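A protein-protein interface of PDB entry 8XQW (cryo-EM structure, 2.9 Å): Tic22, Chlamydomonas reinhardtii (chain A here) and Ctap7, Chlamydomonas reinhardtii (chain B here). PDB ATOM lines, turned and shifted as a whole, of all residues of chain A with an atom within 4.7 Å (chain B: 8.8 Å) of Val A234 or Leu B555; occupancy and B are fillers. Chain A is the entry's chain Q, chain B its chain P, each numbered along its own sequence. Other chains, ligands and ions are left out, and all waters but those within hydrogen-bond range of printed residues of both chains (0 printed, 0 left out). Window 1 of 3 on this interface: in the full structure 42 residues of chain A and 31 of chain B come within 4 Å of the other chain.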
ATOM      1  N   GLN A 220      14.405 -25.813  -9.587  1.00  0.00           N
ATOM      2  CA  GLN A 220      15.421 -25.945 -10.623  1.00  0.00           C
ATOM      3  C   GLN A 220      16.171 -27.250 -10.418  1.00  0.00           C
ATOM      4  O   GLN A 220      16.131 -27.850  -9.341  1.00  0.00           O
ATOM      5  CB  GLN A 220      16.391 -24.760 -10.636  1.00  0.00           C
ATOM      6  CG  GLN A 220      17.275 -24.641  -9.421  1.00  0.00           C
ATOM      7  CD  GLN A 220      18.667 -24.179  -9.784  1.00  0.00           C
ATOM      8  OE1 GLN A 220      19.273 -24.692 -10.727  1.00  0.00           O
ATOM      9  NE2 GLN A 220      19.177 -23.192  -9.055  1.00  0.00           N
ATOM     10  N   LEU A 224      20.710 -29.343 -15.975  1.00  0.00           N
ATOM     11  CA  LEU A 224      19.787 -29.027 -17.054  1.00  0.00           C
ATOM     12  C   LEU A 224      19.876 -27.553 -17.420  1.00  0.00           C
ATOM     13  O   LEU A 224      19.882 -26.677 -16.552  1.00  0.00           O
ATOM     14  CB  LEU A 224      18.358 -29.379 -16.654  1.00  0.00           C
ATOM     15  CG  LEU A 224      17.295 -29.076 -17.708  1.00  0.00           C
ATOM     16  CD1 LEU A 224      17.689 -29.646 -19.062  1.00  0.00           C
ATOM     17  CD2 LEU A 224      15.950 -29.616 -17.264  1.00  0.00           C
ATOM     18  N   THR A 225      19.944 -27.288 -18.721  1.00  0.00           N
ATOM     19  CA  THR A 225      20.021 -25.920 -19.224  1.00  0.00           C
ATOM     20  C   THR A 225      19.526 -25.913 -20.659  1.00  0.00           C
ATOM     21  O   THR A 225      19.901 -26.786 -21.448  1.00  0.00           O
ATOM     22  CB  THR A 225      21.447 -25.383 -19.139  1.00  0.00           C
ATOM     23  OG1 THR A 225      21.536 -24.158 -19.876  1.00  0.00           O
ATOM     24  CG2 THR A 225      22.434 -26.389 -19.706  1.00  0.00           C
ATOM     25  N   GLN A 232      23.800 -20.576 -23.668  1.00  0.00           N
ATOM     26  CA  GLN A 232      23.029 -21.547 -22.900  1.00  0.00           C
ATOM     27  C   GLN A 232      22.363 -20.831 -21.734  1.00  0.00           C
ATOM     28  O   GLN A 232      23.040 -20.195 -20.920  1.00  0.00           O
ATOM     29  CB  GLN A 232      23.929 -22.673 -22.404  1.00  0.00           C
ATOM     30  CG  GLN A 232      24.561 -23.477 -23.513  1.00  0.00           C
ATOM     31  CD  GLN A 232      25.602 -24.445 -23.001  1.00  0.00           C
ATOM     32  OE1 GLN A 232      25.754 -24.626 -21.793  1.00  0.00           O
ATOM     33  NE2 GLN A 232      26.325 -25.081 -23.917  1.00  0.00           N
ATOM     34  N   TYR A 233      21.043 -20.936 -21.656  1.00  0.00           N
ATOM     35  CA  TYR A 233      20.297 -20.369 -20.546  1.00  0.00           C
ATOM     36  C   TYR A 233      19.939 -21.452 -19.541  1.00  0.00           C
ATOM     37  O   TYR A 233      19.921 -22.644 -19.858  1.00  0.00           O
ATOM     38  CB  TYR A 233      19.023 -19.685 -21.040  1.00  0.00           C
ATOM     39  CG  TYR A 233      19.278 -18.483 -21.906  1.00  0.00           C
ATOM     40  CD1 TYR A 233      19.828 -17.330 -21.377  1.00  0.00           C
ATOM     41  CD2 TYR A 233      18.967 -18.499 -23.257  1.00  0.00           C
ATOM     42  CE1 TYR A 233      20.064 -16.229 -22.167  1.00  0.00           C
ATOM     43  CE2 TYR A 233      19.200 -17.405 -24.051  1.00  0.00           C
ATOM     44  CZ  TYR A 233      19.748 -16.273 -23.502  1.00  0.00           C
ATOM     45  OH  TYR A 233      19.981 -15.175 -24.289  1.00  0.00           O
ATOM     46  N   VAL A 234      19.653 -21.024 -18.320  1.00  0.00           N
ATOM     47  CA  VAL A 234      19.219 -21.917 -17.251  1.00  0.00           C
ATOM     48  C   VAL A 234      17.755 -21.616 -16.951  1.00  0.00           C
ATOM     49  O   VAL A 234      17.397 -20.436 -16.788  1.00  0.00           O
ATOM     50  CB  VAL A 234      20.099 -21.764 -15.999  1.00  0.00           C
ATOM     51  CG1 VAL A 234      20.195 -20.307 -15.571  1.00  0.00           C
ATOM     52  CG2 VAL A 234      19.572 -22.626 -14.871  1.00  0.00           C
ATOM     53  N   PRO A 235      16.883 -22.618 -16.915  1.00  0.00           N
ATOM     54  CA  PRO A 235      15.460 -22.371 -16.689  1.00  0.00           C
ATOM     55  C   PRO A 235      15.066 -22.464 -15.225  1.00  0.00           C
ATOM     56  O   PRO A 235      15.724 -23.108 -14.408  1.00  0.00           O
ATOM     57  CB  PRO A 235      14.795 -23.492 -17.498  1.00  0.00           C
ATOM     58  CG  PRO A 235      15.752 -24.612 -17.395  1.00  0.00           C
ATOM     59  CD  PRO A 235      17.137 -24.011 -17.314  1.00  0.00           C
ATOM     60  N   LEU A 236      13.963 -21.795 -14.911  1.00  0.00           N
ATOM     61  CA  LEU A 236      13.344 -21.842 -13.596  1.00  0.00           C
ATOM     62  C   LEU A 236      11.876 -22.204 -13.758  1.00  0.00           C
ATOM     63  O   LEU A 236      11.147 -21.536 -14.500  1.00  0.00           O
ATOM     64  CB  LEU A 236      13.484 -20.509 -12.868  1.00  0.00           C
ATOM     65  CG  LEU A 236      14.587 -20.448 -11.820  1.00  0.00           C
ATOM     66  CD1 LEU A 236      15.944 -20.561 -12.473  1.00  0.00           C
ATOM     67  CD2 LEU A 236      14.479 -19.168 -11.032  1.00  0.00           C
ATOM     68  N   VAL A 329      14.576 -14.581  -4.693  1.00  0.00           N
ATOM     69  CA  VAL A 329      15.181 -14.612  -6.022  1.00  0.00           C
ATOM     70  C   VAL A 329      15.164 -13.225  -6.644  1.00  0.00           C
ATOM     71  O   VAL A 329      16.180 -12.745  -7.153  1.00  0.00           O
ATOM     72  CB  VAL A 329      14.466 -15.639  -6.918  1.00  0.00           C
ATOM     73  CG1 VAL A 329      14.599 -15.253  -8.378  1.00  0.00           C
ATOM     74  CG2 VAL A 329      15.032 -17.020  -6.685  1.00  0.00           C
ATOM     75  N   ALA A 343      25.840 -14.494 -13.510  1.00  0.00           N
ATOM     76  CA  ALA A 343      25.034 -15.695 -13.316  1.00  0.00           C
ATOM     77  C   ALA A 343      23.559 -15.405 -13.556  1.00  0.00           C
ATOM     78  O   ALA A 343      22.883 -16.129 -14.295  1.00  0.00           O
ATOM     79  CB  ALA A 343      25.257 -16.252 -11.910  1.00  0.00           C
ATOM     80  N   TRP A 344      23.045 -14.339 -12.943  1.00  0.00           N
ATOM     81  CA  TRP A 344      21.642 -13.977 -13.092  1.00  0.00           C
ATOM     82  C   TRP A 344      21.289 -13.598 -14.518  1.00  0.00           C
ATOM     83  O   TRP A 344      20.135 -13.759 -14.921  1.00  0.00           O
ATOM     84  CB  TRP A 344      21.294 -12.812 -12.168  1.00  0.00           C
ATOM     85  CG  TRP A 344      21.199 -13.189 -10.731  1.00  0.00           C
ATOM     86  CD1 TRP A 344      21.950 -12.703  -9.707  1.00  0.00           C
ATOM     87  CD2 TRP A 344      20.297 -14.133 -10.155  1.00  0.00           C
ATOM     88  NE1 TRP A 344      21.574 -13.286  -8.527  1.00  0.00           N
ATOM     89  CE2 TRP A 344      20.558 -14.168  -8.775  1.00  0.00           C
ATOM     90  CE3 TRP A 344      19.292 -14.952 -10.673  1.00  0.00           C
ATOM     91  CZ2 TRP A 344      19.853 -14.990  -7.906  1.00  0.00           C
ATOM     92  CZ3 TRP A 344      18.595 -15.764  -9.814  1.00  0.00           C
ATOM     93  CH2 TRP A 344      18.877 -15.778  -8.443  1.00  0.00           C
ATOM     94  N   GLN A 346      21.432 -14.910 -17.177  1.00  0.00           N
ATOM     95  CA  GLN A 346      21.059 -15.994 -18.076  1.00  0.00           C
ATOM     96  C   GLN A 346      19.898 -16.824 -17.549  1.00  0.00           C
ATOM     97  O   GLN A 346      19.660 -17.930 -18.042  1.00  0.00           O
ATOM     98  CB  GLN A 346      22.265 -16.887 -18.355  1.00  0.00           C
ATOM     99  CG  GLN A 346      23.418 -16.159 -19.014  1.00  0.00           C
ATOM    100  CD  GLN A 346      24.741 -16.837 -18.770  1.00  0.00           C
ATOM    101  OE1 GLN A 346      25.661 -16.738 -19.580  1.00  0.00           O
ATOM    102  NE2 GLN A 346      24.844 -17.545 -17.651  1.00  0.00           N
ATOM    103  N   VAL A 347      19.174 -16.322 -16.561  1.00  0.00           N
ATOM    104  CA  VAL A 347      18.015 -17.029 -16.027  1.00  0.00           C
ATOM    105  C   VAL A 347      16.821 -16.794 -16.939  1.00  0.00           C
ATOM    106  O   VAL A 347      16.598 -15.675 -17.412  1.00  0.00           O
ATOM    107  CB  VAL A 347      17.714 -16.561 -14.595  1.00  0.00           C
ATOM    108  CG1 VAL A 347      16.445 -17.211 -14.084  1.00  0.00           C
ATOM    109  CG2 VAL A 347      18.881 -16.868 -13.680  1.00  0.00           C
ATOM    110  N   MET A 348      16.047 -17.847 -17.195  1.00  0.00           N
ATOM    111  CA  MET A 348      14.782 -17.678 -17.894  1.00  0.00           C
ATOM    112  C   MET A 348      13.690 -18.380 -17.102  1.00  0.00           C
ATOM    113  O   MET A 348      13.879 -19.506 -16.640  1.00  0.00           O
ATOM    114  CB  MET A 348      14.854 -18.208 -19.334  1.00  0.00           C
ATOM    115  CG  MET A 348      14.591 -19.692 -19.494  1.00  0.00           C
ATOM    116  SD  MET A 348      15.504 -20.441 -20.855  1.00  0.00           S
ATOM    117  CE  MET A 348      15.370 -19.184 -22.115  1.00  0.00           C
ATOM    118  N   GLY B 536      16.448 -14.338 -21.878  1.00  0.00           N
ATOM    119  CA  GLY B 536      16.108 -15.614 -22.479  1.00  0.00           C
ATOM    120  C   GLY B 536      14.617 -15.897 -22.424  1.00  0.00           C
ATOM    121  O   GLY B 536      13.957 -15.690 -21.407  1.00  0.00           O
ATOM    122  N   ARG B 537      14.090 -16.390 -23.542  1.00  0.00           N
ATOM    123  CA  ARG B 537      12.677 -16.721 -23.685  1.00  0.00           C
ATOM    124  C   ARG B 537      12.536 -18.237 -23.688  1.00  0.00           C
ATOM    125  O   ARG B 537      13.110 -18.917 -24.546  1.00  0.00           O
ATOM    126  CB  ARG B 537      12.105 -16.115 -24.963  1.00  0.00           C
ATOM    127  CG  ARG B 537      10.595 -16.066 -24.986  1.00  0.00           C
ATOM    128  CD  ARG B 537      10.067 -15.011 -24.031  1.00  0.00           C
ATOM    129  NE  ARG B 537      10.482 -13.671 -24.428  1.00  0.00           N
ATOM    130  CZ  ARG B 537      11.331 -12.916 -23.740  1.00  0.00           C
ATOM    131  NH1 ARG B 537      11.856 -13.369 -22.611  1.00  0.00           N
ATOM    132  NH2 ARG B 537      11.651 -11.707 -24.179  1.00  0.00           N
ATOM    133  N   ALA B 538      11.775 -18.764 -22.737  1.00  0.00           N
ATOM    134  CA  ALA B 538      11.677 -20.207 -22.586  1.00  0.00           C
ATOM    135  C   ALA B 538      10.887 -20.814 -23.743  1.00  0.00           C
ATOM    136  O   ALA B 538       9.896 -20.229 -24.192  1.00  0.00           O
ATOM    137  CB  ALA B 538      11.016 -20.562 -21.256  1.00  0.00           C
ATOM    138  N   PRO B 539      11.297 -21.974 -24.249  1.00  0.00           N
ATOM    139  CA  PRO B 539      10.556 -22.632 -25.329  1.00  0.00           C
ATOM    140  C   PRO B 539       9.566 -23.663 -24.807  1.00  0.00           C
ATOM    141  O   PRO B 539       9.671 -24.153 -23.683  1.00  0.00           O
ATOM    142  CB  PRO B 539      11.669 -23.307 -26.140  1.00  0.00           C
ATOM    143  CG  PRO B 539      12.795 -23.523 -25.145  1.00  0.00           C
ATOM    144  CD  PRO B 539      12.525 -22.705 -23.906  1.00  0.00           C
ATOM    145  N   ALA B 544      15.500 -28.068 -26.591  1.00  0.00           N
ATOM    146  CA  ALA B 544      16.688 -27.379 -26.123  1.00  0.00           C
ATOM    147  C   ALA B 544      17.019 -27.711 -24.678  1.00  0.00           C
ATOM    148  O   ALA B 544      18.094 -27.333 -24.202  1.00  0.00           O
ATOM    149  CB  ALA B 544      16.524 -25.864 -26.267  1.00  0.00           C
ATOM    150  N   TYR B 545      16.132 -28.411 -23.977  1.00  0.00           N
ATOM    151  CA  TYR B 545      16.416 -28.864 -22.623  1.00  0.00           C
ATOM    152  C   TYR B 545      17.421 -30.003 -22.742  1.00  0.00           C
ATOM    153  O   TYR B 545      17.075 -31.179 -22.881  1.00  0.00           O
ATOM    154  CB  TYR B 545      15.136 -29.285 -21.918  1.00  0.00           C
ATOM    155  CG  TYR B 545      14.169 -28.143 -21.707  1.00  0.00           C
ATOM    156  CD1 TYR B 545      14.418 -27.170 -20.752  1.00  0.00           C
ATOM    157  CD2 TYR B 545      13.009 -28.038 -22.460  1.00  0.00           C
ATOM    158  CE1 TYR B 545      13.543 -26.125 -20.554  1.00  0.00           C
ATOM    159  CE2 TYR B 545      12.126 -26.996 -22.268  1.00  0.00           C
ATOM    160  CZ  TYR B 545      12.399 -26.044 -21.311  1.00  0.00           C
ATOM    161  OH  TYR B 545      11.524 -25.001 -21.114  1.00  0.00           O
ATOM    162  N   ARG B 551      28.156 -28.145 -15.691  1.00  0.00           N
ATOM    163  CA  ARG B 551      27.828 -27.642 -14.368  1.00  0.00           C
ATOM    164  C   ARG B 551      27.022 -26.361 -14.493  1.00  0.00           C
ATOM    165  O   ARG B 551      27.382 -25.461 -15.255  1.00  0.00           O
ATOM    166  CB  ARG B 551      29.093 -27.391 -13.538  1.00  0.00           C
ATOM    167  CG  ARG B 551      28.820 -26.836 -12.151  1.00  0.00           C
ATOM    168  CD  ARG B 551      27.805 -27.682 -11.387  1.00  0.00           C
ATOM    169  NE  ARG B 551      28.280 -29.040 -11.148  1.00  0.00           N
ATOM    170  CZ  ARG B 551      29.076 -29.389 -10.142  1.00  0.00           C
ATOM    171  NH1 ARG B 551      29.490 -28.476  -9.273  1.00  0.00           N
ATOM    172  NH2 ARG B 551      29.458 -30.652 -10.002  1.00  0.00           N
ATOM    173  N   THR B 552      25.939 -26.283 -13.724  1.00  0.00           N
ATOM    174  CA  THR B 552      25.047 -25.139 -13.714  1.00  0.00           C
ATOM    175  C   THR B 552      25.187 -24.393 -12.396  1.00  0.00           C
ATOM    176  O   THR B 552      25.128 -25.007 -11.324  1.00  0.00           O
ATOM    177  CB  THR B 552      23.590 -25.577 -13.890  1.00  0.00           C
ATOM    178  OG1 THR B 552      23.213 -26.412 -12.792  1.00  0.00           O
ATOM    179  CG2 THR B 552      23.424 -26.357 -15.180  1.00  0.00           C
ATOM    180  N   PRO B 553      25.367 -23.077 -12.439  1.00  0.00           N
ATOM    181  CA  PRO B 553      25.455 -22.315 -11.189  1.00  0.00           C
ATOM    182  C   PRO B 553      24.132 -22.370 -10.446  1.00  0.00           C
ATOM    183  O   PRO B 553      23.068 -22.517 -11.049  1.00  0.00           O
ATOM    184  CB  PRO B 553      25.790 -20.897 -11.658  1.00  0.00           C
ATOM    185  CG  PRO B 553      25.256 -20.829 -13.045  1.00  0.00           C
ATOM    186  CD  PRO B 553      25.391 -22.206 -13.626  1.00  0.00           C
ATOM    187  N   LEU B 554      24.211 -22.276  -9.123  1.00  0.00           N
ATOM    188  CA  LEU B 554      23.019 -22.349  -8.291  1.00  0.00           C
ATOM    189  C   LEU B 554      22.416 -20.957  -8.154  1.00  0.00           C
ATOM    190  O   LEU B 554      23.043 -20.054  -7.592  1.00  0.00           O
ATOM    191  CB  LEU B 554      23.351 -22.936  -6.921  1.00  0.00           C
ATOM    192  CG  LEU B 554      22.285 -22.744  -5.841  1.00  0.00           C
ATOM    193  CD1 LEU B 554      21.003 -23.440  -6.249  1.00  0.00           C
ATOM    194  CD2 LEU B 554      22.771 -23.272  -4.506  1.00  0.00           C
ATOM    195  N   LEU B 555      21.205 -20.784  -8.680  1.00  0.00           N
ATOM    196  CA  LEU B 555      20.496 -19.515  -8.623  1.00  0.00           C
ATOM    197  C   LEU B 555      19.147 -19.638  -7.928  1.00  0.00           C
ATOM    198  O   LEU B 555      18.273 -18.789  -8.127  1.00  0.00           O
ATOM    199  CB  LEU B 555      20.311 -18.950 -10.030  1.00  0.00           C
ATOM    200  CG  LEU B 555      21.570 -18.845 -10.892  1.00  0.00           C
ATOM    201  CD1 LEU B 555      21.522 -19.851 -12.029  1.00  0.00           C
ATOM    202  CD2 LEU B 555      21.732 -17.439 -11.428  1.00  0.00           C
ATOM    203  N   ALA B 556      18.951 -20.688  -7.137  1.00  0.00           N
ATOM    204  CA  ALA B 556      17.743 -20.786  -6.340  1.00  0.00           C
ATOM    205  C   ALA B 556      17.909 -20.013  -5.036  1.00  0.00           C
ATOM    206  O   ALA B 556      19.018 -19.799  -4.541  1.00  0.00           O
ATOM    207  CB  ALA B 556      17.402 -22.246  -6.055  1.00  0.00           C
ATOM    208  N   ALA B 557      16.782 -19.596  -4.477  1.00  0.00           N
ATOM    209  CA  ALA B 557      16.771 -18.776  -3.278  1.00  0.00           C
ATOM    210  C   ALA B 557      16.996 -19.647  -2.048  1.00  0.00           C
ATOM    211  O   ALA B 557      17.420 -20.803  -2.147  1.00  0.00           O
ATOM    212  CB  ALA B 557      15.466 -17.999  -3.182  1.00  0.00           C
ATOM    213  N   GLY B 558      16.715 -19.092  -0.869  1.00  0.00           N
ATOM    214  CA  GLY B 558      16.949 -19.788   0.380  1.00  0.00           C
ATOM    215  C   GLY B 558      16.293 -21.149   0.432  1.00  0.00           C
ATOM    216  O   GLY B 558      15.067 -21.259   0.522  1.00  0.00           O
ATOM    217  N   ASP B 639      30.267 -23.306  -5.469  1.00  0.00           N
ATOM    218  CA  ASP B 639      29.079 -22.649  -4.939  1.00  0.00           C
ATOM    219  C   ASP B 639      29.362 -21.969  -3.606  1.00  0.00           C
ATOM    220  O   ASP B 639      28.752 -20.948  -3.279  1.00  0.00           O
ATOM    221  CB  ASP B 639      27.950 -23.668  -4.800  1.00  0.00           C
ATOM    222  CG  ASP B 639      28.428 -24.980  -4.218  1.00  0.00           C
ATOM    223  OD1 ASP B 639      29.609 -25.057  -3.814  1.00  0.00           O
ATOM    224  OD2 ASP B 639      27.627 -25.936  -4.172  1.00  0.00           O
ATOM    225  N   ALA B 642      30.810 -18.763  -4.493  1.00  0.00           N
ATOM    226  CA  ALA B 642      29.729 -17.875  -4.910  1.00  0.00           C
ATOM    227  C   ALA B 642      29.001 -17.299  -3.704  1.00  0.00           C
ATOM    228  O   ALA B 642      28.692 -16.103  -3.660  1.00  0.00           O
ATOM    229  CB  ALA B 642      28.759 -18.620  -5.826  1.00  0.00           C
ATOM    230  N   ARG B 646      28.945 -13.364  -2.767  1.00  0.00           N
ATOM    231  CA  ARG B 646      27.681 -12.647  -2.713  1.00  0.00           C
ATOM    232  C   ARG B 646      27.493 -11.980  -1.360  1.00  0.00           C
ATOM    233  O   ARG B 646      27.012 -10.843  -1.278  1.00  0.00           O
ATOM    234  CB  ARG B 646      26.536 -13.610  -3.012  1.00  0.00           C
ATOM    235  CG  ARG B 646      25.271 -13.323  -2.242  1.00  0.00           C
ATOM    236  CD  ARG B 646      24.474 -14.588  -2.053  1.00  0.00           C
ATOM    237  NE  ARG B 646      23.890 -15.032  -3.312  1.00  0.00           N
ATOM    238  CZ  ARG B 646      23.118 -16.102  -3.436  1.00  0.00           C
ATOM    239  NH1 ARG B 646      22.835 -16.836  -2.369  1.00  0.00           N
ATOM    240  NH2 ARG B 646      22.627 -16.438  -4.619  1.00  0.00           N
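Printed residues of chain B within 4 Å of Leu A224: Tyr B545 and Thr B552.
Val A234 touches just one residue of chain B: Leu B555.
Leu A236 touches none of the printed residues of chain B.
Arg B551 touches none of the printed residues of chain A.
Of chain A, only Gln A220, Val A234, Val A329, Ala A343, Trp A344 and Val A347 come within 4 Å of Leu B555.
Printed residues of chain A within 4 Å of Ala B556: Gln A220 (3.2 Å).
Among the printed residues, pairs that only touch across the chains: Trp A344 with Leu B555 (3.1 Å), Met A348 with Arg B537 (3.3 Å), Ala A343 with Leu B555 (3.4 Å), Gln A220 with Leu B554 (3.4 Å), Met A348 with Gly B536 (3.4 Å), Val A329 with Ala B557 (3.7 Å), Met A348 with Ala B538 (3.7 Å), Val A347 with Leu B555 (3.7 Å), Leu A224 with Tyr B545 (3.7 Å), Val A234 with Leu B555 (3.8 Å), Leu A224 with Thr B552 (3.8 Å), Tyr A233 with Gly B536 (3.8 Å) and Val A329 with Leu B555 (3.96 Å).
Hydrophobic or aromatic side chains of chain B that line the printed part of chain A: Tyr B545, Leu B554, Leu B555, Ala B556 and Ala B557.
Of the 14 printed residues of chain A, 10 touch a printed residue of chain B.
Among the printed residues, 16 pairs touch across the chains.
O of Pro B539 sits at hydrogen-bond distance from OH of Tyr B545, at 3.3 Å.
The backbone NH of Val A234 sits at hydrogen-bond distance from the backbone carbonyl oxygen of Gln A346 (3.1 Å).
The backbone carbonyl oxygen of Val A234 sits at hydrogen-bond distance from the backbone NH of Met A348 (2.9 Å).
The backbone NH (N) of Leu A236 is in hydrogen-bond range of the backbone carbonyl oxygen (O) of Met A348, at 2.9 Å.
NE2 of Gln A220 sits close to N of Leu B555 (3.2 Å).
N of Ala B556 sits close to NE2 of Gln A220 (3.2 Å).
The backbone carbonyl oxygen (O) of Ala B544 sits close to the backbone carbonyl oxygen (O) of Thr A225, at 3.3 Å.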
